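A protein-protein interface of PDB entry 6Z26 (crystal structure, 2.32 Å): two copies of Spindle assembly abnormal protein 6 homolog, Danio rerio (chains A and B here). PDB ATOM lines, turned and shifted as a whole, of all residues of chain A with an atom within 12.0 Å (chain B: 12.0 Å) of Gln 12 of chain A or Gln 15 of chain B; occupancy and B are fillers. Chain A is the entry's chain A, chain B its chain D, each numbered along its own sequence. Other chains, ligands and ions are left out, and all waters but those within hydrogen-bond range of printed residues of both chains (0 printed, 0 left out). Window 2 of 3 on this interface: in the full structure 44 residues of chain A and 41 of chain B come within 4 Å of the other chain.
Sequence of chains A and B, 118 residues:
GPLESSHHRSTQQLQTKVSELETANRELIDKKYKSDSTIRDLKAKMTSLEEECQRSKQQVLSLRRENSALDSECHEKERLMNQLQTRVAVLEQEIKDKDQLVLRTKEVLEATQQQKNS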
ATOM      1  N   GLN A  12       7.677  26.792  11.625  1.00  0.00           N
ATOM      2  CA  GLN A  12       8.123  28.083  12.143  1.00  0.00           C
ATOM      3  C   GLN A  12       7.446  28.453  13.501  1.00  0.00           C
ATOM      4  O   GLN A  12       6.918  29.553  13.672  1.00  0.00           O
ATOM      5  CB  GLN A  12       7.969  29.185  11.071  1.00  0.00           C
ATOM      6  CG  GLN A  12       9.008  30.310  11.170  1.00  0.00           C
ATOM      7  CD  GLN A  12       8.878  31.381  10.102  1.00  0.00           C
ATOM      8  OE1 GLN A  12       7.778  31.748   9.653  1.00  0.00           O
ATOM      9  NE2 GLN A  12      10.016  31.926   9.689  1.00  0.00           N
ATOM     10  N   GLN A  13       7.489  27.506  14.458  1.00  0.00           N
ATOM     11  CA  GLN A  13       7.014  27.622  15.846  1.00  0.00           C
ATOM     12  C   GLN A  13       7.895  26.734  16.749  1.00  0.00           C
ATOM     13  O   GLN A  13       7.710  26.670  17.976  1.00  0.00           O
ATOM     14  CB  GLN A  13       5.529  27.229  15.964  1.00  0.00           C
ATOM     15  CG  GLN A  13       4.896  27.617  17.318  1.00  0.00           C
ATOM     16  CD  GLN A  13       3.415  27.351  17.467  1.00  0.00           C
ATOM     17  OE1 GLN A  13       2.683  27.098  16.503  1.00  0.00           O
ATOM     18  NE2 GLN A  13       2.941  27.411  18.700  1.00  0.00           N
ATOM     19  N   LEU A  14       8.877  26.054  16.108  1.00  0.00           N
ATOM     20  CA  LEU A  14       9.785  25.119  16.784  1.00  0.00           C
ATOM     21  C   LEU A  14      11.254  25.463  16.584  1.00  0.00           C
ATOM     22  O   LEU A  14      11.729  25.602  15.444  1.00  0.00           O
ATOM     23  CB  LEU A  14       9.504  23.646  16.404  1.00  0.00           C
ATOM     24  CG  LEU A  14       8.144  23.056  16.844  1.00  0.00           C
ATOM     25  CD1 LEU A  14       7.891  21.712  16.193  1.00  0.00           C
ATOM     26  CD2 LEU A  14       8.039  22.939  18.367  1.00  0.00           C
ATOM     27  N   GLN A  15      11.961  25.581  17.718  1.00  0.00           N
ATOM     28  CA  GLN A  15      13.376  25.868  17.854  1.00  0.00           C
ATOM     29  C   GLN A  15      14.151  24.532  17.968  1.00  0.00           C
ATOM     30  O   GLN A  15      15.158  24.475  18.684  1.00  0.00           O
ATOM     31  CB  GLN A  15      13.634  26.762  19.100  1.00  0.00           C
ATOM     32  CG  GLN A  15      13.019  28.174  19.043  1.00  0.00           C
ATOM     33  CD  GLN A  15      13.311  29.030  20.264  1.00  0.00           C
ATOM     34  OE1 GLN A  15      13.027  28.654  21.406  1.00  0.00           O
ATOM     35  NE2 GLN A  15      13.868  30.218  20.045  1.00  0.00           N
ATOM     36  N   THR A  16      13.683  23.451  17.285  1.00  0.00           N
ATOM     37  CA  THR A  16      14.405  22.161  17.319  1.00  0.00           C
ATOM     38  C   THR A  16      15.655  22.270  16.477  1.00  0.00           C
ATOM     39  O   THR A  16      16.562  21.437  16.603  1.00  0.00           O
ATOM     40  CB  THR A  16      13.616  20.977  16.750  1.00  0.00           C
ATOM     41  OG1 THR A  16      12.851  21.394  15.611  1.00  0.00           O
ATOM     42  CG2 THR A  16      12.784  20.244  17.795  1.00  0.00           C
ATOM     43  N   LYS A  17      15.663  23.258  15.561  1.00  0.00           N
ATOM     44  CA  LYS A  17      16.789  23.558  14.707  1.00  0.00           C
ATOM     45  C   LYS A  17      17.921  24.073  15.599  1.00  0.00           C
ATOM     46  O   LYS A  17      19.063  23.794  15.284  1.00  0.00           O
ATOM     47  CB  LYS A  17      16.409  24.582  13.626  1.00  0.00           C
ATOM     48  CG  LYS A  17      17.501  24.750  12.577  1.00  0.00           C
ATOM     49  CD  LYS A  17      17.173  25.754  11.515  1.00  0.00           C
ATOM     50  CE  LYS A  17      18.382  25.976  10.641  1.00  0.00           C
ATOM     51  NZ  LYS A  17      18.055  26.744   9.413  1.00  0.00           N
ATOM     52  N   VAL A  18      17.612  24.758  16.731  1.00  0.00           N
ATOM     53  CA  VAL A  18      18.613  25.267  17.687  1.00  0.00           C
ATOM     54  C   VAL A  18      19.371  24.099  18.360  1.00  0.00           C
ATOM     55  O   VAL A  18      20.607  24.084  18.342  1.00  0.00           O
ATOM     56  CB  VAL A  18      18.018  26.289  18.699  1.00  0.00           C
ATOM     57  CG1 VAL A  18      18.998  26.617  19.824  1.00  0.00           C
ATOM     58  CG2 VAL A  18      17.590  27.565  17.990  1.00  0.00           C
ATOM     59  N   SER A  19      18.618  23.101  18.886  1.00  0.00           N
ATOM     60  CA  SER A  19      19.143  21.894  19.539  1.00  0.00           C
ATOM     61  C   SER A  19      20.012  21.045  18.598  1.00  0.00           C
ATOM     62  O   SER A  19      20.952  20.397  19.062  1.00  0.00           O
ATOM     63  CB  SER A  19      17.995  21.055  20.085  1.00  0.00           C
ATOM     64  OG  SER A  19      17.278  21.777  21.073  1.00  0.00           O
ATOM     65  N   LEU A  21      21.468  22.474  15.732  1.00  0.00           N
ATOM     66  CA  LEU A  21      22.473  23.432  15.301  1.00  0.00           C
ATOM     67  C   LEU A  21      23.512  23.618  16.407  1.00  0.00           C
ATOM     68  O   LEU A  21      24.621  24.049  16.121  1.00  0.00           O
ATOM     69  CB  LEU A  21      21.715  24.732  14.974  1.00  0.00           C
ATOM     70  CG  LEU A  21      22.351  25.953  14.292  1.00  0.00           C
ATOM     71  CD1 LEU A  21      23.240  25.603  13.113  1.00  0.00           C
ATOM     72  CD2 LEU A  21      21.258  26.886  13.768  1.00  0.00           C
ATOM     73  N   GLU A  22      23.166  23.262  17.657  1.00  0.00           N
ATOM     74  CA  GLU A  22      24.087  23.327  18.787  1.00  0.00           C
ATOM     75  C   GLU A  22      24.853  22.005  18.939  1.00  0.00           C
ATOM     76  O   GLU A  22      26.030  22.032  19.313  1.00  0.00           O
ATOM     77  CB  GLU A  22      23.383  23.773  20.081  1.00  0.00           C
ATOM     78  CG  GLU A  22      23.312  25.290  20.172  1.00  0.00           C
ATOM     79  CD  GLU A  22      22.619  25.927  21.365  1.00  0.00           C
ATOM     80  OE1 GLU A  22      21.578  25.394  21.813  1.00  0.00           O
ATOM     81  OE2 GLU A  22      23.106  26.984  21.832  1.00  0.00           O
ATOM     82  N   LEU B  14      14.033  34.999  19.507  1.00  0.00           N
ATOM     83  CA  LEU B  14      13.357  33.763  19.116  1.00  0.00           C
ATOM     84  C   LEU B  14      14.108  33.065  17.964  1.00  0.00           C
ATOM     85  O   LEU B  14      14.998  32.254  18.225  1.00  0.00           O
ATOM     86  CB  LEU B  14      11.864  34.012  18.759  1.00  0.00           C
ATOM     87  CG  LEU B  14      10.908  34.504  19.870  1.00  0.00           C
ATOM     88  CD1 LEU B  14       9.504  34.772  19.309  1.00  0.00           C
ATOM     89  CD2 LEU B  14      10.819  33.513  21.031  1.00  0.00           C
ATOM     90  N   GLN B  15      13.775  33.412  16.697  1.00  0.00           N
ATOM     91  CA  GLN B  15      14.400  32.886  15.468  1.00  0.00           C
ATOM     92  C   GLN B  15      15.747  33.590  15.263  1.00  0.00           C
ATOM     93  O   GLN B  15      16.467  33.327  14.295  1.00  0.00           O
ATOM     94  CB  GLN B  15      13.499  33.145  14.236  1.00  0.00           C
ATOM     95  CG  GLN B  15      12.005  32.823  14.414  1.00  0.00           C
ATOM     96  CD  GLN B  15      11.129  33.271  13.255  1.00  0.00           C
ATOM     97  OE1 GLN B  15      11.595  33.621  12.157  1.00  0.00           O
ATOM     98  NE2 GLN B  15       9.820  33.257  13.474  1.00  0.00           N
ATOM     99  N   THR B  16      16.049  34.515  16.184  1.00  0.00           N
ATOM    100  CA  THR B  16      17.232  35.366  16.262  1.00  0.00           C
ATOM    101  C   THR B  16      18.494  34.559  16.576  1.00  0.00           C
ATOM    102  O   THR B  16      19.517  34.765  15.917  1.00  0.00           O
ATOM    103  CB  THR B  16      16.968  36.521  17.257  1.00  0.00           C
ATOM    104  OG1 THR B  16      16.463  35.982  18.485  1.00  0.00           O
ATOM    105  CG2 THR B  16      15.954  37.548  16.715  1.00  0.00           C
ATOM    106  N   LYS B  17      18.420  33.625  17.554  1.00  0.00           N
ATOM    107  CA  LYS B  17      19.557  32.768  17.941  1.00  0.00           C
ATOM    108  C   LYS B  17      19.878  31.687  16.891  1.00  0.00           C
ATOM    109  O   LYS B  17      21.003  31.183  16.860  1.00  0.00           O
ATOM    110  CB  LYS B  17      19.362  32.163  19.345  1.00  0.00           C
ATOM    111  CG  LYS B  17      19.688  33.148  20.464  1.00  0.00           C
ATOM    112  CD  LYS B  17      18.809  32.960  21.694  1.00  0.00           C
ATOM    113  CE  LYS B  17      18.768  34.216  22.536  1.00  0.00           C
ATOM    114  NZ  LYS B  17      18.606  33.915  23.983  1.00  0.00           N
ATOM    115  N   VAL B  18      18.893  31.362  16.024  1.00  0.00           N
ATOM    116  CA  VAL B  18      18.995  30.396  14.923  1.00  0.00           C
ATOM    117  C   VAL B  18      20.013  30.940  13.902  1.00  0.00           C
ATOM    118  O   VAL B  18      20.843  30.185  13.394  1.00  0.00           O
ATOM    119  CB  VAL B  18      17.601  30.138  14.264  1.00  0.00           C
ATOM    120  CG1 VAL B  18      17.668  29.034  13.212  1.00  0.00           C
ATOM    121  CG2 VAL B  18      16.537  29.810  15.305  1.00  0.00           C
ATOM    122  N   SER B  19      19.954  32.259  13.639  1.00  0.00           N
ATOM    123  CA  SER B  19      20.823  32.963  12.697  1.00  0.00           C
ATOM    124  C   SER B  19      22.269  33.060  13.175  1.00  0.00           C
ATOM    125  O   SER B  19      23.181  32.883  12.366  1.00  0.00           O
ATOM    126  CB  SER B  19      20.262  34.347  12.384  1.00  0.00           C
ATOM    127  OG  SER B  19      19.083  34.229  11.605  1.00  0.00           O
ATOM    128  N   GLU B  20      22.473  33.334  14.485  1.00  0.00           N
ATOM    129  CA  GLU B  20      23.790  33.448  15.139  1.00  0.00           C
ATOM    130  C   GLU B  20      24.539  32.115  15.098  1.00  0.00           C
ATOM    131  O   GLU B  20      25.777  32.069  15.125  1.00  0.00           O
ATOM    132  CB  GLU B  20      23.603  33.846  16.610  1.00  0.00           C
ATOM    133  CG  GLU B  20      23.494  35.338  16.852  1.00  0.00           C
ATOM    134  CD  GLU B  20      23.640  35.726  18.309  1.00  0.00           C
ATOM    135  OE1 GLU B  20      24.789  35.742  18.812  1.00  0.00           O
ATOM    136  OE2 GLU B  20      22.605  36.019  18.951  1.00  0.00           O
ATOM    137  N   LEU B  21      23.755  31.034  15.091  1.00  0.00           N
ATOM    138  CA  LEU B  21      24.212  29.661  15.075  1.00  0.00           C
ATOM    139  C   LEU B  21      24.470  29.178  13.638  1.00  0.00           C
ATOM    140  O   LEU B  21      25.359  28.349  13.432  1.00  0.00           O
ATOM    141  CB  LEU B  21      23.167  28.796  15.778  1.00  0.00           C
ATOM    142  CG  LEU B  21      23.241  28.589  17.286  1.00  0.00           C
ATOM    143  CD1 LEU B  21      22.013  27.864  17.744  1.00  0.00           C
ATOM    144  CD2 LEU B  21      24.485  27.777  17.699  1.00  0.00           C
ATOM    145  N   GLU B  22      23.721  29.720  12.647  1.00  0.00           N
ATOM    146  CA  GLU B  22      23.892  29.388  11.227  1.00  0.00           C
ATOM    147  C   GLU B  22      25.223  29.934  10.711  1.00  0.00           C
ATOM    148  O   GLU B  22      25.901  29.259   9.940  1.00  0.00           O
ATOM    149  CB  GLU B  22      22.735  29.936  10.388  1.00  0.00           C
ATOM    150  CG  GLU B  22      21.524  29.015  10.328  1.00  0.00           C
ATOM    151  CD  GLU B  22      20.280  29.588   9.676  1.00  0.00           C
ATOM    152  OE1 GLU B  22      20.416  30.272   8.636  1.00  0.00           O
ATOM    153  OE2 GLU B  22      19.167  29.324  10.185  1.00  0.00           O
ATOM    154  N   THR B  23      25.593  31.152  11.170  1.00  0.00           N
ATOM    155  CA  THR B  23      26.831  31.886  10.881  1.00  0.00           C
ATOM    156  C   THR B  23      28.014  31.143  11.516  1.00  0.00           C
ATOM    157  O   THR B  23      29.068  31.007  10.886  1.00  0.00           O
ATOM    158  CB  THR B  23      26.751  33.317  11.472  1.00  0.00           C
ATOM    159  OG1 THR B  23      25.501  33.932  11.137  1.00  0.00           O
ATOM    160  CG2 THR B  23      27.913  34.208  11.033  1.00  0.00           C
ATOM    161  N   ALA B  24      27.836  30.684  12.768  1.00  0.00           N
ATOM    162  CA  ALA B  24      28.839  29.955  13.530  1.00  0.00           C
ATOM    163  C   ALA B  24      29.191  28.643  12.830  1.00  0.00           C
ATOM    164  O   ALA B  24      30.380  28.353  12.657  1.00  0.00           O
ATOM    165  CB  ALA B  24      28.333  29.699  14.945  1.00  0.00           C
ATOM    166  N   ARG B  26      28.500  27.640   9.409  1.00  0.00           N
ATOM    167  CA  ARG B  26      29.062  27.929   8.093  1.00  0.00           C
ATOM    168  C   ARG B  26      30.527  28.343   8.215  1.00  0.00           C
ATOM    169  O   ARG B  26      31.348  27.911   7.408  1.00  0.00           O
ATOM    170  CB  ARG B  26      28.243  28.996   7.355  1.00  0.00           C
ATOM    171  CG  ARG B  26      26.996  28.429   6.686  1.00  0.00           C
ATOM    172  CD  ARG B  26      26.056  29.523   6.210  1.00  0.00           C
ATOM    173  NE  ARG B  26      24.660  29.244   6.554  1.00  0.00           N
ATOM    174  CZ  ARG B  26      23.629  30.001   6.195  1.00  0.00           C
ATOM    175  NH1 ARG B  26      23.832  31.093   5.460  1.00  0.00           N
ATOM    176  NH2 ARG B  26      22.397  29.676   6.544  1.00  0.00           N
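The backbone NH (N) of Leu 14 of chain B lies within hydrogen-bond range of the side-chain hydroxyl (OG1) of Thr 16 of chain B (2.8 Å).
OE1 of Glu 22 of chain B is in salt-bridge range of NH2 of Arg 26 of chain B, 2.9 Å away.
Gln 15 of chain A touches Leu 14 of chain B, but with the chains exchanged Leu 14 of chain A does not touch Gln 15 of chain B (7.3 Å).
Lys 17 of chain A touches Val 18 of chain B, but with the chains exchanged Val 18 of chain A does not touch Lys 17 of chain B (4.8 Å).
Val 18 of chain A touches Leu 21 of chain B, and with the chains exchanged Leu 21 of chain A touches Val 18 of chain B.
Leu 21 of chain A touches Glu 22 of chain B, and with the chains exchanged Glu 22 of chain A touches Leu 21 of chain B.
Positions printed for both chains: 14, 15, 16, 17, 18, 19, 21 and 22.
Of the 10 printed residues of chain A, 6 touch a printed residue of chain B.
Printed residues of chain A that touch a printed residue of chain B: Gln 12, Gln 15, Lys 17, Val 18, Leu 21 and Glu 22.
Hydrophobic or aromatic side chains of chain A that line the printed part of chain B: Val 18 and Leu 21.
Along chain B the printed residues that touch a printed residue of chain A span positions 14 to 22.
Among the printed residues, 10 pairs touch across the chains.
Among the printed residues, Asp or Glu carboxylates within 4 Å of a Lys or Arg side-chain nitrogen of the other chain: Lys 17 of chain A with Glu 22 of chain B (2.9 Å).
NE2 of Gln 15 of chain A sits at hydrogen-bond distance from O of Leu 14 of chain B, at 3.0 Å.
NZ of Lys 17 of chain A lies within salt-bridge range of OE2 of Glu 22 of chain B (2.9 Å).
The side-chain amide nitrogen of Gln 12 of chain A sits at hydrogen-bond distance from the side-chain amide oxygen of Gln 15 of chain B.
Among the printed residues, pairs that only touch across the chains: Leu 21 of chain A with Leu 21 of chain B, Leu 21 of chain A with Val 18 of chain B, Val 18 of chain A with Val 18 of chain B, Glu 22 of chain A with Leu 21 of chain B, Lys 17 of chain A with Val 18 of chain B, Val 18 of chain A with Leu 21 of chain B and Leu 21 of chain A with Glu 22 of chain B.
Printed residues of chain B within 4 Å of Gln 12 of chain A: Gln 15 (3.4 Å).
Of chain A, only Gln 12 (3.4 Å) comes within 4 Å of Gln 15 of chain B.
No residue of chain B comes within 4 Å of Gln 13 of chain A.
Leu 14 of chain B touches just one residue of chain A: Gln 15 (3.0 Å).
No residue of chain A comes within 4 Å of Thr 16 of chain B.
Of chain A, only Lys 17 (3.7 Å), Val 18 (3.7 Å) and Leu 21 (3.3 Å) come within 4 Å of Val 18 of chain B.
Printed residues of chain B within 4 Å of Glu 22 of chain A: Leu 21 (3.7 Å).
Printed residues of chain B within 4 Å of Gln 15 of chain A: Leu 14 (3.0 Å).
Of the printed residues of chain B, Val 18 of chain A touches Val 18 (3.7 Å) and Leu 21 (3.9 Å).
Glu 20 of chain B touches none of the printed residues of chain A.
The nearest residue of chain B that does not touch Gln 12 of chain A is Leu 14 of chain B (8.1 Å).
The nearest printed residue of chain B that does not touch Leu 21 of chain A is Lys 17 of chain B (5.3 Å).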
